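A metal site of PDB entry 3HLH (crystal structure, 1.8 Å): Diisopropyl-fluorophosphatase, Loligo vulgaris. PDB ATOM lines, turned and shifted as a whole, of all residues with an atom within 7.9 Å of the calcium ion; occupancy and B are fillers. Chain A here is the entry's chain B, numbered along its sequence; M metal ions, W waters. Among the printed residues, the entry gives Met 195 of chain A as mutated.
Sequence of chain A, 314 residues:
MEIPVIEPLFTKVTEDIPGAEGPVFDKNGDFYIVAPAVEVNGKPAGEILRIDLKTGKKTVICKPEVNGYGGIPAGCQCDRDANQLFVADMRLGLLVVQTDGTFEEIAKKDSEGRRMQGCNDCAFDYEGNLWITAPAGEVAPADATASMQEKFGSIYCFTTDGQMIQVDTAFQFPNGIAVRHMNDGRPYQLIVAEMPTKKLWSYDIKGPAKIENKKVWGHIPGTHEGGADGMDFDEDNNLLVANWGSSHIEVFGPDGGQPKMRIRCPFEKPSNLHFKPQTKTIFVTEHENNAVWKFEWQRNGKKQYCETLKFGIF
The side-chain amide nitrogen (ND2) of Asn 175 sits close to the side-chain sulfur (SD) of Met 195, at 3.7 Å. The backbone carbonyl oxygen of Asn 175 sits at hydrogen-bond distance from the side-chain hydroxyl of Thr 133, 2.7 Å away. ND2 of Asn 272 is in hydrogen-bond range of OE1 of Glu 21. N of Gly 176 lies close to O of Asp 229 (3.0 Å). The backbone carbonyl oxygen of Asn 120 is in hydrogen-bond range of the backbone NH of Gly 75 (3.0 Å). The backbone NH of Asn 120 sits at hydrogen-bond distance from the backbone carbonyl oxygen of Thr 133 (2.8 Å). The side-chain amide nitrogen (ND2) of Asn 120 sits at hydrogen-bond distance from the side-chain sulfur (SD) of Met 90 (3.8 Å).
The nearest printed residue that does not touch the calcium ion is Asn 272 (4.4 Å).
The side-chain amide oxygen (OD1) of Asn 175 binds the calcium ion (2.3 Å). The calcium ion is bound by the side-chain carboxylate (OE2) of Glu 21. The calcium ion is bound by the side-chain carboxylate (OD1) of Asp 229, 2.4 Å away. The calcium ion is bound by water W2, 2.4 Å away. The calcium ion is bound by OD1 of Asn 120, at 2.4 Å. The calcium ion is bound by water W1. The calcium ion has six donor atoms within binding distance.
Water W2 lies within hydrogen-bond range of the side-chain carboxylate of Asp 121 (2.7 Å), the backbone NH of Gly 230 (3.4 Å) and the backbone NH of Gly 176 (3.4 Å).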
ATOM      1  N   GLY A  19      21.721 -20.639   8.726  1.00  0.00           N
ATOM      2  CA  GLY A  19      20.430 -21.255   8.990  1.00  0.00           C
ATOM      3  C   GLY A  19      20.186 -22.507   8.176  1.00  0.00           C
ATOM      4  O   GLY A  19      19.034 -22.908   7.998  1.00  0.00           O
ATOM      5  N   ALA A  20      21.254 -23.121   7.672  1.00  0.00           N
ATOM      6  CA  ALA A  20      21.170 -24.327   6.850  1.00  0.00           C
ATOM      7  C   ALA A  20      19.907 -25.141   7.129  1.00  0.00           C
ATOM      8  O   ALA A  20      19.693 -25.646   8.236  1.00  0.00           O
ATOM      9  CB  ALA A  20      22.424 -25.194   7.076  1.00  0.00           C
ATOM     10  N   GLU A  21      19.083 -25.295   6.100  1.00  0.00           N
ATOM     11  CA  GLU A  21      17.810 -26.009   6.214  1.00  0.00           C
ATOM     12  C   GLU A  21      17.330 -26.573   4.875  1.00  0.00           C
ATOM     13  O   GLU A  21      18.059 -26.554   3.882  1.00  0.00           O
ATOM     14  CB  GLU A  21      16.757 -25.040   6.766  1.00  0.00           C
ATOM     15  CG  GLU A  21      16.331 -25.308   8.191  1.00  0.00           C
ATOM     16  CD  GLU A  21      15.254 -26.366   8.297  1.00  0.00           C
ATOM     17  OE1 GLU A  21      15.122 -27.169   7.349  1.00  0.00           O
ATOM     18  OE2 GLU A  21      14.541 -26.397   9.327  1.00  0.00           O
ATOM     19  N   GLY A  22      16.104 -27.086   4.887  1.00  0.00           N
ATOM     20  CA  GLY A  22      15.470 -27.633   3.700  1.00  0.00           C
ATOM     21  C   GLY A  22      16.248 -28.514   2.733  1.00  0.00           C
ATOM     22  O   GLY A  22      16.204 -28.271   1.529  1.00  0.00           O
ATOM     23  N   PRO A  36      17.886 -19.720   5.163  1.00  0.00           N
ATOM     24  CA  PRO A  36      16.904 -18.740   5.631  1.00  0.00           C
ATOM     25  C   PRO A  36      17.450 -17.606   6.486  1.00  0.00           C
ATOM     26  O   PRO A  36      16.870 -16.534   6.520  1.00  0.00           O
ATOM     27  CB  PRO A  36      15.910 -19.608   6.418  1.00  0.00           C
ATOM     28  CG  PRO A  36      16.782 -20.712   6.945  1.00  0.00           C
ATOM     29  CD  PRO A  36      17.623 -21.057   5.733  1.00  0.00           C
ATOM     30  N   ALA A  74      12.821 -21.827   4.028  1.00  0.00           N
ATOM     31  CA  ALA A  74      13.181 -22.697   5.140  1.00  0.00           C
ATOM     32  C   ALA A  74      12.968 -24.194   4.973  1.00  0.00           C
ATOM     33  O   ALA A  74      13.574 -24.985   5.697  1.00  0.00           O
ATOM     34  CB  ALA A  74      12.458 -22.219   6.398  1.00  0.00           C
ATOM     35  N   GLY A  75      12.108 -24.592   4.043  1.00  0.00           N
ATOM     36  CA  GLY A  75      11.844 -26.017   3.833  1.00  0.00           C
ATOM     37  C   GLY A  75      11.520 -26.312   2.382  1.00  0.00           C
ATOM     38  O   GLY A  75      10.963 -25.458   1.688  1.00  0.00           O
ATOM     39  N   MET A  90       9.369 -18.473   5.295  1.00  0.00           N
ATOM     40  CA  MET A  90       8.894 -17.791   6.493  1.00  0.00           C
ATOM     41  C   MET A  90       8.397 -16.367   6.263  1.00  0.00           C
ATOM     42  O   MET A  90       7.668 -15.826   7.086  1.00  0.00           O
ATOM     43  CB  MET A  90       9.990 -17.786   7.565  1.00  0.00           C
ATOM     44  CG  MET A  90      10.320 -19.167   8.137  1.00  0.00           C
ATOM     45  SD  MET A  90       9.042 -19.800   9.266  1.00  0.00           S
ATOM     46  CE  MET A  90       9.523 -19.001  10.806  1.00  0.00           C
ATOM     47  N   CYS A 119       5.630 -19.763   6.013  1.00  0.00           N
ATOM     48  CA  CYS A 119       5.749 -21.209   6.166  1.00  0.00           C
ATOM     49  C   CYS A 119       7.164 -21.684   6.502  1.00  0.00           C
ATOM     50  O   CYS A 119       8.145 -21.003   6.191  1.00  0.00           O
ATOM     51  CB  CYS A 119       5.252 -21.893   4.885  1.00  0.00           C
ATOM     52  SG  CYS A 119       3.505 -21.492   4.520  1.00  0.00           S
ATOM     53  N   ASN A 120       7.264 -22.840   7.147  1.00  0.00           N
ATOM     54  CA  ASN A 120       8.566 -23.369   7.555  1.00  0.00           C
ATOM     55  C   ASN A 120       8.989 -24.644   6.828  1.00  0.00           C
ATOM     56  O   ASN A 120      10.095 -24.719   6.299  1.00  0.00           O
ATOM     57  CB  ASN A 120       8.576 -23.604   9.073  1.00  0.00           C
ATOM     58  CG  ASN A 120       9.938 -23.984   9.597  1.00  0.00           C
ATOM     59  OD1 ASN A 120      10.448 -25.067   9.326  1.00  0.00           O
ATOM     60  ND2 ASN A 120      10.552 -23.073  10.369  1.00  0.00           N
ATOM     61  N   ASP A 121       8.120 -25.650   6.803  1.00  0.00           N
ATOM     62  CA  ASP A 121       8.438 -26.910   6.127  1.00  0.00           C
ATOM     63  C   ASP A 121       7.193 -27.485   5.478  1.00  0.00           C
ATOM     64  O   ASP A 121       6.074 -27.048   5.740  1.00  0.00           O
ATOM     65  CB  ASP A 121       9.020 -27.920   7.122  1.00  0.00           C
ATOM     66  CG  ASP A 121      10.031 -28.871   6.473  1.00  0.00           C
ATOM     67  OD1 ASP A 121      10.103 -28.928   5.237  1.00  0.00           O
ATOM     68  OD2 ASP A 121      10.757 -29.564   7.216  1.00  0.00           O
ATOM     69  N   CYS A 122       7.385 -28.476   4.604  1.00  0.00           N
ATOM     70  CA  CYS A 122       6.244 -29.081   3.932  1.00  0.00           C
ATOM     71  C   CYS A 122       6.540 -30.531   3.591  1.00  0.00           C
ATOM     72  O   CYS A 122       7.697 -30.947   3.535  1.00  0.00           O
ATOM     73  CB  CYS A 122       5.888 -28.288   2.666  1.00  0.00           C
ATOM     74  SG  CYS A 122       7.273 -27.940   1.515  1.00  0.00           S
ATOM     75  N   THR A 133       3.655 -26.421   7.269  1.00  0.00           N
ATOM     76  CA  THR A 133       3.609 -25.822   8.600  1.00  0.00           C
ATOM     77  C   THR A 133       3.846 -24.322   8.444  1.00  0.00           C
ATOM     78  O   THR A 133       4.661 -23.898   7.620  1.00  0.00           O
ATOM     79  CB  THR A 133       4.682 -26.408   9.554  1.00  0.00           C
ATOM     80  OG1 THR A 133       5.992 -26.165   9.012  1.00  0.00           O
ATOM     81  CG2 THR A 133       4.468 -27.904   9.749  1.00  0.00           C
ATOM     82  N   PRO A 135       4.540 -21.449  11.134  1.00  0.00           N
ATOM     83  CA  PRO A 135       4.803 -20.903  12.465  1.00  0.00           C
ATOM     84  C   PRO A 135       4.926 -19.378  12.511  1.00  0.00           C
ATOM     85  O   PRO A 135       4.850 -18.771  13.568  1.00  0.00           O
ATOM     86  CB  PRO A 135       6.109 -21.584  12.847  1.00  0.00           C
ATOM     87  CG  PRO A 135       6.851 -21.569  11.534  1.00  0.00           C
ATOM     88  CD  PRO A 135       5.773 -22.031  10.560  1.00  0.00           C
ATOM     89  N   PHE A 173       4.400 -22.762  17.322  1.00  0.00           N
ATOM     90  CA  PHE A 173       5.510 -22.942  16.389  1.00  0.00           C
ATOM     91  C   PHE A 173       5.642 -24.323  15.756  1.00  0.00           C
ATOM     92  O   PHE A 173       6.553 -25.097  16.080  1.00  0.00           O
ATOM     93  CB  PHE A 173       6.833 -22.557  17.066  1.00  0.00           C
ATOM     94  CG  PHE A 173       7.856 -22.010  16.102  1.00  0.00           C
ATOM     95  CD1 PHE A 173       8.618 -22.874  15.316  1.00  0.00           C
ATOM     96  CD2 PHE A 173       8.020 -20.638  15.962  1.00  0.00           C
ATOM     97  CE1 PHE A 173       9.545 -22.362  14.407  1.00  0.00           C
ATOM     98  CE2 PHE A 173       8.950 -20.120  15.045  1.00  0.00           C
ATOM     99  CZ  PHE A 173       9.705 -20.982  14.271  1.00  0.00           C
ATOM    100  N   PRO A 174       4.707 -24.646  14.843  1.00  0.00           N
ATOM    101  CA  PRO A 174       4.753 -25.945  14.160  1.00  0.00           C
ATOM    102  C   PRO A 174       5.998 -25.866  13.274  1.00  0.00           C
ATOM    103  O   PRO A 174       6.314 -24.809  12.729  1.00  0.00           O
ATOM    104  CB  PRO A 174       3.459 -25.948  13.359  1.00  0.00           C
ATOM    105  CG  PRO A 174       3.216 -24.493  13.109  1.00  0.00           C
ATOM    106  CD  PRO A 174       3.511 -23.892  14.443  1.00  0.00           C
ATOM    107  N   ASN A 175       6.708 -26.971  13.133  1.00  0.00           N
ATOM    108  CA  ASN A 175       7.929 -26.938  12.348  1.00  0.00           C
ATOM    109  C   ASN A 175       7.992 -28.092  11.358  1.00  0.00           C
ATOM    110  O   ASN A 175       7.474 -27.983  10.246  1.00  0.00           O
ATOM    111  CB  ASN A 175       9.136 -26.974  13.311  1.00  0.00           C
ATOM    112  CG  ASN A 175      10.390 -26.375  12.696  1.00  0.00           C
ATOM    113  OD1 ASN A 175      10.727 -26.680  11.556  1.00  0.00           O
ATOM    114  ND2 ASN A 175      11.085 -25.543  13.464  1.00  0.00           N
ATOM    115  N   GLY A 176       8.595 -29.204  11.759  1.00  0.00           N
ATOM    116  CA  GLY A 176       8.665 -30.349  10.873  1.00  0.00           C
ATOM    117  C   GLY A 176       7.297 -30.984  10.636  1.00  0.00           C
ATOM    118  O   GLY A 176       6.366 -30.782  11.417  1.00  0.00           O
ATOM    119  N   ILE A 177       7.183 -31.741   9.559  1.00  0.00           N
ATOM    120  CA  ILE A 177       5.911 -32.380   9.223  1.00  0.00           C
ATOM    121  C   ILE A 177       6.170 -33.587   8.323  1.00  0.00           C
ATOM    122  O   ILE A 177       7.129 -33.601   7.557  1.00  0.00           O
ATOM    123  CB  ILE A 177       4.964 -31.357   8.534  1.00  0.00           C
ATOM    124  CG1 ILE A 177       3.588 -31.978   8.265  1.00  0.00           C
ATOM    125  CG2 ILE A 177       5.587 -30.841   7.237  1.00  0.00           C
ATOM    126  CD1 ILE A 177       2.557 -30.964   7.803  1.00  0.00           C
ATOM    127  N   MET A 195       7.468 -27.555  17.930  1.00  0.00           N
ATOM    128  CA  MET A 195       8.813 -27.445  18.503  1.00  0.00           C
ATOM    129  C   MET A 195       9.028 -27.216  20.005  1.00  0.00           C
ATOM    130  O   MET A 195       9.440 -28.135  20.710  1.00  0.00           O
ATOM    131  CB  MET A 195       9.626 -26.427  17.697  1.00  0.00           C
ATOM    132  CG  MET A 195      11.085 -26.391  18.108  1.00  0.00           C
ATOM    133  SD  MET A 195      12.082 -25.374  17.014  1.00  0.00           S
ATOM    134  CE  MET A 195      13.120 -26.608  16.257  1.00  0.00           C
ATOM    135  N   ALA A 228      11.698 -30.616  18.334  1.00  0.00           N
ATOM    136  CA  ALA A 228      11.609 -31.221  17.012  1.00  0.00           C
ATOM    137  C   ALA A 228      11.630 -30.193  15.897  1.00  0.00           C
ATOM    138  O   ALA A 228      10.877 -29.214  15.921  1.00  0.00           O
ATOM    139  CB  ALA A 228      10.341 -32.069  16.914  1.00  0.00           C
ATOM    140  N   ASP A 229      12.525 -30.389  14.933  1.00  0.00           N
ATOM    141  CA  ASP A 229      12.609 -29.499  13.787  1.00  0.00           C
ATOM    142  C   ASP A 229      12.162 -30.342  12.587  1.00  0.00           C
ATOM    143  O   ASP A 229      10.998 -30.740  12.527  1.00  0.00           O
ATOM    144  CB  ASP A 229      14.048 -28.999  13.582  1.00  0.00           C
ATOM    145  CG  ASP A 229      14.116 -27.706  12.777  1.00  0.00           C
ATOM    146  OD1 ASP A 229      13.249 -27.505  11.894  1.00  0.00           O
ATOM    147  OD2 ASP A 229      15.039 -26.889  13.008  1.00  0.00           O
ATOM    148  N   GLY A 230      13.071 -30.644  11.664  1.00  0.00           N
ATOM    149  CA  GLY A 230      12.702 -31.429  10.488  1.00  0.00           C
ATOM    150  C   GLY A 230      12.543 -32.917  10.726  1.00  0.00           C
ATOM    151  O   GLY A 230      13.079 -33.459  11.687  1.00  0.00           O
ATOM    152  N   MET A 231      11.792 -33.591   9.847  1.00  0.00           N
ATOM    153  CA  MET A 231      11.565 -35.032  10.001  1.00  0.00           C
ATOM    154  C   MET A 231      11.340 -35.754   8.678  1.00  0.00           C
ATOM    155  O   MET A 231      11.020 -35.135   7.663  1.00  0.00           O
ATOM    156  CB  MET A 231      10.339 -35.277  10.883  1.00  0.00           C
ATOM    157  CG  MET A 231       9.041 -34.704  10.311  1.00  0.00           C
ATOM    158  SD  MET A 231       7.567 -35.008  11.315  1.00  0.00           S
ATOM    159  CE  MET A 231       8.159 -34.439  12.943  1.00  0.00           C
ATOM    160  N   TRP A 244      16.502 -30.309  17.648  1.00  0.00           N
ATOM    161  CA  TRP A 244      17.330 -29.109  17.743  1.00  0.00           C
ATOM    162  C   TRP A 244      17.683 -28.769  19.188  1.00  0.00           C
ATOM    163  O   TRP A 244      16.798 -28.580  20.017  1.00  0.00           O
ATOM    164  CB  TRP A 244      16.563 -27.937  17.111  1.00  0.00           C
ATOM    165  CG  TRP A 244      17.391 -26.736  16.726  1.00  0.00           C
ATOM    166  CD1 TRP A 244      17.797 -26.390  15.462  1.00  0.00           C
ATOM    167  CD2 TRP A 244      17.833 -25.678  17.586  1.00  0.00           C
ATOM    168  NE1 TRP A 244      18.454 -25.183  15.481  1.00  0.00           N
ATOM    169  CE2 TRP A 244      18.488 -24.723  16.773  1.00  0.00           C
ATOM    170  CE3 TRP A 244      17.735 -25.437  18.971  1.00  0.00           C
ATOM    171  CZ2 TRP A 244      19.045 -23.546  17.291  1.00  0.00           C
ATOM    172  CZ3 TRP A 244      18.292 -24.261  19.489  1.00  0.00           C
ATOM    173  CH2 TRP A 244      18.935 -23.335  18.649  1.00  0.00           C
ATOM    174  N   SER A 271      18.883 -29.388  12.271  1.00  0.00           N
ATOM    175  CA  SER A 271      17.657 -28.682  11.902  1.00  0.00           C
ATOM    176  C   SER A 271      16.757 -29.502  10.995  1.00  0.00           C
ATOM    177  O   SER A 271      15.543 -29.436  11.110  1.00  0.00           O
ATOM    178  CB  SER A 271      18.006 -27.354  11.211  1.00  0.00           C
ATOM    179  OG  SER A 271      18.739 -27.578  10.012  1.00  0.00           O
ATOM    180  N   ASN A 272      17.350 -30.272  10.095  1.00  0.00           N
ATOM    181  CA  ASN A 272      16.551 -31.073   9.190  1.00  0.00           C
ATOM    182  C   ASN A 272      17.388 -32.184   8.599  1.00  0.00           C
ATOM    183  O   ASN A 272      18.586 -32.267   8.838  1.00  0.00           O
ATOM    184  CB  ASN A 272      15.987 -30.194   8.057  1.00  0.00           C
ATOM    185  CG  ASN A 272      14.589 -30.600   7.656  1.00  0.00           C
ATOM    186  OD1 ASN A 272      14.256 -31.791   7.645  1.00  0.00           O
ATOM    187  ND2 ASN A 272      13.754 -29.621   7.299  1.00  0.00           N
ATOM    188  N   THR A 285      21.215 -31.030   8.008  1.00  0.00           N
ATOM    189  CA  THR A 285      21.552 -29.614   8.080  1.00  0.00           C
ATOM    190  C   THR A 285      21.570 -29.305   9.580  1.00  0.00           C
ATOM    191  O   THR A 285      20.866 -29.941  10.346  1.00  0.00           O
ATOM    192  CB  THR A 285      20.492 -28.727   7.358  1.00  0.00           C
ATOM    193  OG1 THR A 285      19.173 -29.092   7.786  1.00  0.00           O
ATOM    194  CG2 THR A 285      20.597 -28.916   5.842  1.00  0.00           C
ATOM    195  N   HIS A 287      22.399 -25.976  12.715  1.00  0.00           N
ATOM    196  CA  HIS A 287      22.626 -24.571  13.015  1.00  0.00           C
ATOM    197  C   HIS A 287      23.756 -24.224  13.972  1.00  0.00           C
ATOM    198  O   HIS A 287      23.952 -23.048  14.278  1.00  0.00           O
ATOM    199  CB  HIS A 287      21.312 -23.971  13.517  1.00  0.00           C
ATOM    200  CG  HIS A 287      20.203 -24.015  12.502  1.00  0.00           C
ATOM    201  ND1 HIS A 287      18.892 -23.761  12.823  1.00  0.00           N
ATOM    202  CD2 HIS A 287      20.225 -24.267  11.171  1.00  0.00           C
ATOM    203  CE1 HIS A 287      18.149 -23.861  11.735  1.00  0.00           C
ATOM    204  NE2 HIS A 287      18.935 -24.169  10.719  1.00  0.00           N
HETATM  205 CA    CA M   1      12.326 -26.455   9.976  1.00  0.00          CA
HETATM  206  O   HOH W   1      12.214 -26.347   7.484  1.00  0.00           O
HETATM  207  O   HOH W   2      11.243 -28.568   9.666  1.00  0.00           O
